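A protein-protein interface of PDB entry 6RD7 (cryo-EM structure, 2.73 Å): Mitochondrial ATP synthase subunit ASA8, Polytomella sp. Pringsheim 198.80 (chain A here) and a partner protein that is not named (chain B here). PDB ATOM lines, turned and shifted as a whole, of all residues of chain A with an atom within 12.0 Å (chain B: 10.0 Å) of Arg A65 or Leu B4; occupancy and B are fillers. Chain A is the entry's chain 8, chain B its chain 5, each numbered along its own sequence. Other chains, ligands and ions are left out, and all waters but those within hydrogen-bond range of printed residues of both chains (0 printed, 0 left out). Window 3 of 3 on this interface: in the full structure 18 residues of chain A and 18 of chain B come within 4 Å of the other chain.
NH1 of Arg A65 is in hydrogen-bond range of O of Pro B5, 2.6 Å away.
The side-chain carboxylate (OD2) of Asp A62 lies within hydrogen-bond range of the backbone NH (N) of Leu B8 (2.9 Å).
The side-chain hydroxyl of Ser B7 lies within hydrogen-bond range of the side-chain carboxylate of Asp A62 (3.1 Å).
OD2 of Asp A62 lies within hydrogen-bond range of N of Gln B9.
The backbone carbonyl oxygen (O) of Glu B6 is in hydrogen-bond range of the guanidinium group (NH1) of Arg A65 (3.5 Å).
Leu B8 touches Tyr A58.
Tyr A58 touches Gln B9.
CA of Gly A59 touches NE2 of Gln B9, at 3.4 Å.
Arg A65 touches Leu B4 (NH2 to CG, 3.6 Å).
The guanidinium group (NH1) of Arg A65 lies within salt-bridge range of the side-chain carboxylate (OD1) of Asp A62, 3.7 Å away.
The side-chain hydroxyl of Ser B7 is in hydrogen-bond range of the backbone NH of Gln B10, at 3.5 Å.
Printed residues of chain B within 4 Å of Tyr A58: Leu B8 (3.3 Å) and Gln B9 (3.8 Å).
Of the printed residues of chain B, Gly A59 touches Gln B9 (3.4 Å).
No residue of chain B comes within 4 Å of Leu A64.
Arg A65 touches just these residues of chain B: Leu B4, Pro B5 and Glu B6.
No residue of chain B comes within 4 Å of Asp A66.
No residue of chain B comes within 4 Å of Ser A67.
No residue of chain B comes within 4 Å of Gly A68.
No residue of chain A comes within 4 Å of Lys B2.
No residue of chain A comes within 4 Å of Leu B3.
Pro B5 touches just one residue of chain A: Arg A65 (2.6 Å).
Printed residues of chain A within 4 Å of Glu B6: Arg A65 (3.5 Å).
Of the printed residues of chain A, Leu B8 touches Tyr A58 (3.3 Å) and Asp A62 (2.9 Å).
Of the printed residues of chain A, Gln B9 touches Tyr A58 (3.8 Å), Gly A59 (3.4 Å) and Asp A62 (2.7 Å).
Of the 11 printed residues of chain B, 6 touch a printed residue of chain A.
Hydrophobic or aromatic side chains of chain B that line the printed part of chain A: Leu B4 and Leu B8.
Of the 19 printed residues of chain A, 4 touch a printed residue of chain B.
Hydrophobic or aromatic side chains of chain A within 4 Å of the printed part of chain B: Tyr A58.
Among the printed residues, no Asp or Glu carboxylate lies within 4 Å of a Lys or Arg side-chain nitrogen of the other chain.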
ATOM      1  N   THR A  56      14.322  13.253 -18.071  1.00  0.00           N
ATOM      2  CA  THR A  56      13.236  13.675 -18.953  1.00  0.00           C
ATOM      3  C   THR A  56      12.855  15.137 -18.720  1.00  0.00           C
ATOM      4  O   THR A  56      12.707  15.913 -19.677  1.00  0.00           O
ATOM      5  CB  THR A  56      12.032  12.757 -18.743  1.00  0.00           C
ATOM      6  OG1 THR A  56      12.383  11.424 -19.124  1.00  0.00           O
ATOM      7  CG2 THR A  56      10.848  13.210 -19.568  1.00  0.00           C
ATOM      8  N   LEU A  57      12.732  15.538 -17.451  1.00  0.00           N
ATOM      9  CA  LEU A  57      12.350  16.907 -17.122  1.00  0.00           C
ATOM     10  C   LEU A  57      13.432  17.899 -17.526  1.00  0.00           C
ATOM     11  O   LEU A  57      13.129  19.001 -18.000  1.00  0.00           O
ATOM     12  CB  LEU A  57      12.052  17.010 -15.628  1.00  0.00           C
ATOM     13  CG  LEU A  57      11.959  18.392 -14.991  1.00  0.00           C
ATOM     14  CD1 LEU A  57      10.628  19.033 -15.324  1.00  0.00           C
ATOM     15  CD2 LEU A  57      12.152  18.301 -13.492  1.00  0.00           C
ATOM     16  N   TYR A  58      14.698  17.512 -17.401  1.00  0.00           N
ATOM     17  CA  TYR A  58      15.768  18.434 -17.754  1.00  0.00           C
ATOM     18  C   TYR A  58      15.945  18.503 -19.263  1.00  0.00           C
ATOM     19  O   TYR A  58      16.376  19.530 -19.794  1.00  0.00           O
ATOM     20  CB  TYR A  58      17.065  18.030 -17.057  1.00  0.00           C
ATOM     21  CG  TYR A  58      17.189  18.568 -15.649  1.00  0.00           C
ATOM     22  CD1 TYR A  58      16.140  18.456 -14.747  1.00  0.00           C
ATOM     23  CD2 TYR A  58      18.350  19.185 -15.222  1.00  0.00           C
ATOM     24  CE1 TYR A  58      16.240  18.938 -13.477  1.00  0.00           C
ATOM     25  CE2 TYR A  58      18.460  19.672 -13.942  1.00  0.00           C
ATOM     26  CZ  TYR A  58      17.398  19.542 -13.080  1.00  0.00           C
ATOM     27  OH  TYR A  58      17.478  20.018 -11.807  1.00  0.00           O
ATOM     28  N   GLY A  59      15.571  17.439 -19.976  1.00  0.00           N
ATOM     29  CA  GLY A  59      15.477  17.538 -21.423  1.00  0.00           C
ATOM     30  C   GLY A  59      14.369  18.472 -21.868  1.00  0.00           C
ATOM     31  O   GLY A  59      14.526  19.219 -22.839  1.00  0.00           O
ATOM     32  N   ILE A  60      13.242  18.459 -21.148  1.00  0.00           N
ATOM     33  CA  ILE A  60      12.154  19.401 -21.420  1.00  0.00           C
ATOM     34  C   ILE A  60      12.604  20.840 -21.165  1.00  0.00           C
ATOM     35  O   ILE A  60      12.325  21.747 -21.961  1.00  0.00           O
ATOM     36  CB  ILE A  60      10.916  19.027 -20.583  1.00  0.00           C
ATOM     37  CG1 ILE A  60      10.311  17.721 -21.090  1.00  0.00           C
ATOM     38  CG2 ILE A  60       9.868  20.118 -20.614  1.00  0.00           C
ATOM     39  CD1 ILE A  60       9.212  17.186 -20.214  1.00  0.00           C
ATOM     40  N   LEU A  61      13.337  21.062 -20.072  1.00  0.00           N
ATOM     41  CA  LEU A  61      13.820  22.406 -19.756  1.00  0.00           C
ATOM     42  C   LEU A  61      14.880  22.875 -20.749  1.00  0.00           C
ATOM     43  O   LEU A  61      14.937  24.063 -21.092  1.00  0.00           O
ATOM     44  CB  LEU A  61      14.367  22.446 -18.332  1.00  0.00           C
ATOM     45  CG  LEU A  61      13.363  22.208 -17.205  1.00  0.00           C
ATOM     46  CD1 LEU A  61      14.016  22.428 -15.854  1.00  0.00           C
ATOM     47  CD2 LEU A  61      12.150  23.099 -17.367  1.00  0.00           C
ATOM     48  N   ASP A  62      15.713  21.954 -21.240  1.00  0.00           N
ATOM     49  CA  ASP A  62      16.673  22.302 -22.284  1.00  0.00           C
ATOM     50  C   ASP A  62      15.972  22.638 -23.592  1.00  0.00           C
ATOM     51  O   ASP A  62      16.411  23.529 -24.327  1.00  0.00           O
ATOM     52  CB  ASP A  62      17.660  21.156 -22.495  1.00  0.00           C
ATOM     53  CG  ASP A  62      18.836  21.222 -21.553  1.00  0.00           C
ATOM     54  OD1 ASP A  62      19.160  22.332 -21.085  1.00  0.00           O
ATOM     55  OD2 ASP A  62      19.442  20.166 -21.287  1.00  0.00           O
ATOM     56  N   GLY A  63      14.876  21.936 -23.895  1.00  0.00           N
ATOM     57  CA  GLY A  63      14.088  22.281 -25.067  1.00  0.00           C
ATOM     58  C   GLY A  63      13.440  23.648 -24.956  1.00  0.00           C
ATOM     59  O   GLY A  63      13.379  24.394 -25.937  1.00  0.00           O
ATOM     60  N   LEU A  64      12.970  24.000 -23.755  1.00  0.00           N
ATOM     61  CA  LEU A  64      12.409  25.333 -23.527  1.00  0.00           C
ATOM     62  C   LEU A  64      13.469  26.417 -23.684  1.00  0.00           C
ATOM     63  O   LEU A  64      13.213  27.469 -24.285  1.00  0.00           O
ATOM     64  CB  LEU A  64      11.782  25.414 -22.137  1.00  0.00           C
ATOM     65  CG  LEU A  64      10.525  24.600 -21.843  1.00  0.00           C
ATOM     66  CD1 LEU A  64       9.900  25.073 -20.549  1.00  0.00           C
ATOM     67  CD2 LEU A  64       9.535  24.699 -22.985  1.00  0.00           C
ATOM     68  N   ARG A  65      14.670  26.165 -23.158  1.00  0.00           N
ATOM     69  CA  ARG A  65      15.764  27.125 -23.277  1.00  0.00           C
ATOM     70  C   ARG A  65      16.192  27.306 -24.730  1.00  0.00           C
ATOM     71  O   ARG A  65      16.447  28.431 -25.184  1.00  0.00           O
ATOM     72  CB  ARG A  65      16.942  26.661 -22.424  1.00  0.00           C
ATOM     73  CG  ARG A  65      18.086  27.635 -22.348  1.00  0.00           C
ATOM     74  CD  ARG A  65      18.699  27.618 -20.972  1.00  0.00           C
ATOM     75  NE  ARG A  65      19.480  26.410 -20.731  1.00  0.00           N
ATOM     76  CZ  ARG A  65      20.806  26.362 -20.758  1.00  0.00           C
ATOM     77  NH1 ARG A  65      21.434  25.219 -20.524  1.00  0.00           N
ATOM     78  NH2 ARG A  65      21.506  27.456 -21.020  1.00  0.00           N
ATOM     79  N   ASP A  66      16.241  26.207 -25.486  1.00  0.00           N
ATOM     80  CA  ASP A  66      16.637  26.292 -26.886  1.00  0.00           C
ATOM     81  C   ASP A  66      15.564  26.971 -27.730  1.00  0.00           C
ATOM     82  O   ASP A  66      15.885  27.713 -28.664  1.00  0.00           O
ATOM     83  CB  ASP A  66      16.948  24.901 -27.429  1.00  0.00           C
ATOM     84  CG  ASP A  66      17.533  24.943 -28.819  1.00  0.00           C
ATOM     85  OD1 ASP A  66      18.709  25.335 -28.955  1.00  0.00           O
ATOM     86  OD2 ASP A  66      16.818  24.586 -29.778  1.00  0.00           O
ATOM     87  N   SER A  67      14.286  26.753 -27.404  1.00  0.00           N
ATOM     88  CA  SER A  67      13.222  27.427 -28.140  1.00  0.00           C
ATOM     89  C   SER A  67      13.190  28.918 -27.826  1.00  0.00           C
ATOM     90  O   SER A  67      12.884  29.734 -28.702  1.00  0.00           O
ATOM     91  CB  SER A  67      11.873  26.783 -27.831  1.00  0.00           C
ATOM     92  OG  SER A  67      11.500  27.008 -26.486  1.00  0.00           O
ATOM     93  N   GLY A  68      13.528  29.295 -26.591  1.00  0.00           N
ATOM     94  CA  GLY A  68      13.654  30.710 -26.273  1.00  0.00           C
ATOM     95  C   GLY A  68      14.813  31.372 -26.995  1.00  0.00           C
ATOM     96  O   GLY A  68      14.692  32.506 -27.478  1.00  0.00           O
ATOM     97  N   LYS A  69      15.947  30.667 -27.094  1.00  0.00           N
ATOM     98  CA  LYS A  69      17.078  31.182 -27.863  1.00  0.00           C
ATOM     99  C   LYS A  69      16.738  31.300 -29.345  1.00  0.00           C
ATOM    100  O   LYS A  69      17.148  32.259 -30.007  1.00  0.00           O
ATOM    101  CB  LYS A  69      18.302  30.287 -27.676  1.00  0.00           C
ATOM    102  CG  LYS A  69      19.107  30.577 -26.430  1.00  0.00           C
ATOM    103  CD  LYS A  69      20.431  29.842 -26.461  1.00  0.00           C
ATOM    104  CE  LYS A  69      20.230  28.353 -26.252  1.00  0.00           C
ATOM    105  NZ  LYS A  69      21.517  27.609 -26.222  1.00  0.00           N
ATOM    106  N   LYS A  70      15.967  30.345 -29.873  1.00  0.00           N
ATOM    107  CA  LYS A  70      15.557  30.397 -31.273  1.00  0.00           C
ATOM    108  C   LYS A  70      14.596  31.550 -31.532  1.00  0.00           C
ATOM    109  O   LYS A  70      14.680  32.213 -32.573  1.00  0.00           O
ATOM    110  CB  LYS A  70      14.915  29.072 -31.675  1.00  0.00           C
ATOM    111  CG  LYS A  70      14.637  28.938 -33.155  1.00  0.00           C
ATOM    112  CD  LYS A  70      14.568  27.481 -33.563  1.00  0.00           C
ATOM    113  CE  LYS A  70      13.662  27.294 -34.763  1.00  0.00           C
ATOM    114  NZ  LYS A  70      12.348  27.962 -34.563  1.00  0.00           N
ATOM    115  N   LYS A  71      13.684  31.807 -30.589  1.00  0.00           N
ATOM    116  CA  LYS A  71      12.760  32.927 -30.724  1.00  0.00           C
ATOM    117  C   LYS A  71      13.495  34.261 -30.690  1.00  0.00           C
ATOM    118  O   LYS A  71      13.201  35.156 -31.494  1.00  0.00           O
ATOM    119  CB  LYS A  71      11.703  32.871 -29.622  1.00  0.00           C
ATOM    120  CG  LYS A  71      10.626  33.928 -29.743  1.00  0.00           C
ATOM    121  CD  LYS A  71       9.532  33.730 -28.713  1.00  0.00           C
ATOM    122  CE  LYS A  71       9.989  34.170 -27.334  1.00  0.00           C
ATOM    123  NZ  LYS A  71      10.192  35.642 -27.257  1.00  0.00           N
ATOM    124  N   ALA A  72      14.474  34.402 -29.791  1.00  0.00           N
ATOM    125  CA  ALA A  72      15.254  35.638 -29.742  1.00  0.00           C
ATOM    126  C   ALA A  72      16.126  35.802 -30.984  1.00  0.00           C
ATOM    127  O   ALA A  72      16.305  36.923 -31.478  1.00  0.00           O
ATOM    128  CB  ALA A  72      16.108  35.672 -28.478  1.00  0.00           C
ATOM    129  N   TYR A  73      16.643  34.692 -31.518  1.00  0.00           N
ATOM    130  CA  TYR A  73      17.439  34.730 -32.744  1.00  0.00           C
ATOM    131  C   TYR A  73      16.602  35.171 -33.938  1.00  0.00           C
ATOM    132  O   TYR A  73      17.036  36.013 -34.735  1.00  0.00           O
ATOM    133  CB  TYR A  73      18.040  33.348 -32.995  1.00  0.00           C
ATOM    134  CG  TYR A  73      19.274  33.322 -33.861  1.00  0.00           C
ATOM    135  CD1 TYR A  73      20.540  33.379 -33.298  1.00  0.00           C
ATOM    136  CD2 TYR A  73      19.173  33.208 -35.240  1.00  0.00           C
ATOM    137  CE1 TYR A  73      21.674  33.341 -34.085  1.00  0.00           C
ATOM    138  CE2 TYR A  73      20.302  33.172 -36.036  1.00  0.00           C
ATOM    139  CZ  TYR A  73      21.547  33.241 -35.452  1.00  0.00           C
ATOM    140  OH  TYR A  73      22.673  33.204 -36.238  1.00  0.00           O
ATOM    141  N   ASP A  74      15.391  34.625 -34.068  1.00  0.00           N
ATOM    142  CA  ASP A  74      14.520  35.003 -35.176  1.00  0.00           C
ATOM    143  C   ASP A  74      14.022  36.436 -35.029  1.00  0.00           C
ATOM    144  O   ASP A  74      13.852  37.145 -36.028  1.00  0.00           O
ATOM    145  CB  ASP A  74      13.344  34.033 -35.271  1.00  0.00           C
ATOM    146  CG  ASP A  74      13.771  32.648 -35.696  1.00  0.00           C
ATOM    147  OD1 ASP A  74      14.945  32.479 -36.077  1.00  0.00           O
ATOM    148  OD2 ASP A  74      12.933  31.724 -35.645  1.00  0.00           O
ATOM    149  N   MET B   1      29.744  34.994 -13.854  1.00  0.00           N
ATOM    150  CA  MET B   1      29.893  33.714 -13.174  1.00  0.00           C
ATOM    151  C   MET B   1      29.033  32.665 -13.875  1.00  0.00           C
ATOM    152  O   MET B   1      27.944  32.974 -14.356  1.00  0.00           O
ATOM    153  CB  MET B   1      29.512  33.839 -11.692  1.00  0.00           C
ATOM    154  CG  MET B   1      29.769  32.583 -10.869  1.00  0.00           C
ATOM    155  SD  MET B   1      29.429  32.765  -9.111  1.00  0.00           S
ATOM    156  CE  MET B   1      27.642  32.661  -9.108  1.00  0.00           C
ATOM    157  N   LYS B   2      29.544  31.436 -13.954  1.00  0.00           N
ATOM    158  CA  LYS B   2      28.773  30.331 -14.506  1.00  0.00           C
ATOM    159  C   LYS B   2      27.612  29.990 -13.580  1.00  0.00           C
ATOM    160  O   LYS B   2      27.805  29.700 -12.397  1.00  0.00           O
ATOM    161  CB  LYS B   2      29.682  29.108 -14.700  1.00  0.00           C
ATOM    162  CG  LYS B   2      29.050  27.872 -15.362  1.00  0.00           C
ATOM    163  CD  LYS B   2      28.595  26.817 -14.348  1.00  0.00           C
ATOM    164  CE  LYS B   2      29.761  26.196 -13.603  1.00  0.00           C
ATOM    165  NZ  LYS B   2      29.298  25.223 -12.575  1.00  0.00           N
ATOM    166  N   LEU B   3      26.398  30.042 -14.118  1.00  0.00           N
ATOM    167  CA  LEU B   3      25.244  29.545 -13.385  1.00  0.00           C
ATOM    168  C   LEU B   3      24.545  28.436 -14.148  1.00  0.00           C
ATOM    169  O   LEU B   3      24.363  27.327 -13.639  1.00  0.00           O
ATOM    170  CB  LEU B   3      24.263  30.674 -13.120  1.00  0.00           C
ATOM    171  CG  LEU B   3      24.765  31.699 -12.125  1.00  0.00           C
ATOM    172  CD1 LEU B   3      23.894  32.865 -12.226  1.00  0.00           C
ATOM    173  CD2 LEU B   3      24.640  31.121 -10.749  1.00  0.00           C
ATOM    174  N   LEU B   4      24.172  28.730 -15.344  1.00  0.00           N
ATOM    175  CA  LEU B   4      23.428  27.836 -16.202  1.00  0.00           C
ATOM    176  C   LEU B   4      24.397  27.029 -17.039  1.00  0.00           C
ATOM    177  O   LEU B   4      25.334  27.604 -17.609  1.00  0.00           O
ATOM    178  CB  LEU B   4      22.497  28.637 -17.102  1.00  0.00           C
ATOM    179  CG  LEU B   4      21.120  28.092 -17.464  1.00  0.00           C
ATOM    180  CD1 LEU B   4      20.421  27.524 -16.261  1.00  0.00           C
ATOM    181  CD2 LEU B   4      20.302  29.219 -18.043  1.00  0.00           C
ATOM    182  N   PRO B   5      24.237  25.721 -17.132  1.00  0.00           N
ATOM    183  CA  PRO B   5      25.169  24.906 -17.907  1.00  0.00           C
ATOM    184  C   PRO B   5      24.874  25.011 -19.398  1.00  0.00           C
ATOM    185  O   PRO B   5      23.912  25.640 -19.831  1.00  0.00           O
ATOM    186  CB  PRO B   5      24.908  23.499 -17.384  1.00  0.00           C
ATOM    187  CG  PRO B   5      23.484  23.524 -16.990  1.00  0.00           C
ATOM    188  CD  PRO B   5      23.221  24.896 -16.456  1.00  0.00           C
ATOM    189  N   GLU B   6      25.740  24.378 -20.185  1.00  0.00           N
ATOM    190  CA  GLU B   6      25.505  24.263 -21.617  1.00  0.00           C
ATOM    191  C   GLU B   6      24.326  23.339 -21.892  1.00  0.00           C
ATOM    192  O   GLU B   6      23.508  23.592 -22.782  1.00  0.00           O
ATOM    193  CB  GLU B   6      26.777  23.765 -22.299  1.00  0.00           C
ATOM    194  CG  GLU B   6      26.691  23.608 -23.798  1.00  0.00           C
ATOM    195  CD  GLU B   6      27.850  22.800 -24.345  1.00  0.00           C
ATOM    196  OE1 GLU B   6      28.942  22.853 -23.743  1.00  0.00           O
ATOM    197  OE2 GLU B   6      27.672  22.112 -25.370  1.00  0.00           O
ATOM    198  N   SER B   7      24.218  22.263 -21.118  1.00  0.00           N
ATOM    199  CA  SER B   7      23.089  21.346 -21.178  1.00  0.00           C
ATOM    200  C   SER B   7      22.697  20.960 -19.762  1.00  0.00           C
ATOM    201  O   SER B   7      23.538  20.494 -18.988  1.00  0.00           O
ATOM    202  CB  SER B   7      23.428  20.103 -21.994  1.00  0.00           C
ATOM    203  OG  SER B   7      22.262  19.354 -22.272  1.00  0.00           O
ATOM    204  N   LEU B   8      21.427  21.164 -19.422  1.00  0.00           N
ATOM    205  CA  LEU B   8      20.939  20.722 -18.123  1.00  0.00           C
ATOM    206  C   LEU B   8      20.754  19.212 -18.099  1.00  0.00           C
ATOM    207  O   LEU B   8      20.990  18.566 -17.071  1.00  0.00           O
ATOM    208  CB  LEU B   8      19.627  21.426 -17.790  1.00  0.00           C
ATOM    209  CG  LEU B   8      19.726  22.851 -17.257  1.00  0.00           C
ATOM    210  CD1 LEU B   8      18.459  23.613 -17.579  1.00  0.00           C
ATOM    211  CD2 LEU B   8      19.983  22.845 -15.765  1.00  0.00           C
ATOM    212  N   GLN B   9      20.349  18.632 -19.230  1.00  0.00           N
ATOM    213  CA  GLN B   9      20.069  17.204 -19.276  1.00  0.00           C
ATOM    214  C   GLN B   9      21.347  16.385 -19.232  1.00  0.00           C
ATOM    215  O   GLN B   9      21.375  15.308 -18.631  1.00  0.00           O
ATOM    216  CB  GLN B   9      19.265  16.863 -20.525  1.00  0.00           C
ATOM    217  CG  GLN B   9      18.639  15.496 -20.468  1.00  0.00           C
ATOM    218  CD  GLN B   9      18.099  15.047 -21.795  1.00  0.00           C
ATOM    219  OE1 GLN B   9      18.729  15.242 -22.831  1.00  0.00           O
ATOM    220  NE2 GLN B   9      16.926  14.435 -21.777  1.00  0.00           N
ATOM    221  N   GLN B  10      22.418  16.885 -19.851  1.00  0.00           N
ATOM    222  CA  GLN B  10      23.698  16.186 -19.811  1.00  0.00           C
ATOM    223  C   GLN B  10      24.265  16.168 -18.399  1.00  0.00           C
ATOM    224  O   GLN B  10      24.815  15.159 -17.948  1.00  0.00           O
ATOM    225  CB  GLN B  10      24.679  16.848 -20.775  1.00  0.00           C
ATOM    226  CG  GLN B  10      26.038  16.197 -20.847  1.00  0.00           C
ATOM    227  CD  GLN B  10      27.129  17.200 -21.125  1.00  0.00           C
ATOM    228  OE1 GLN B  10      26.974  18.390 -20.863  1.00  0.00           O
ATOM    229  NE2 GLN B  10      28.243  16.728 -21.662  1.00  0.00           N
ATOM    230  N   GLU B  11      24.075  17.259 -17.661  1.00  0.00           N
ATOM    231  CA  GLU B  11      24.602  17.339 -16.306  1.00  0.00           C
ATOM    232  C   GLU B  11      23.756  16.520 -15.336  1.00  0.00           C
ATOM    233  O   GLU B  11      24.287  15.869 -14.425  1.00  0.00           O
ATOM    234  CB  GLU B  11      24.668  18.800 -15.882  1.00  0.00           C
ATOM    235  CG  GLU B  11      25.425  19.036 -14.617  1.00  0.00           C
ATOM    236  CD  GLU B  11      25.456  20.493 -14.240  1.00  0.00           C
ATOM    237  OE1 GLU B  11      24.859  21.302 -14.970  1.00  0.00           O
ATOM    238  OE2 GLU B  11      26.068  20.825 -13.211  1.00  0.00           O
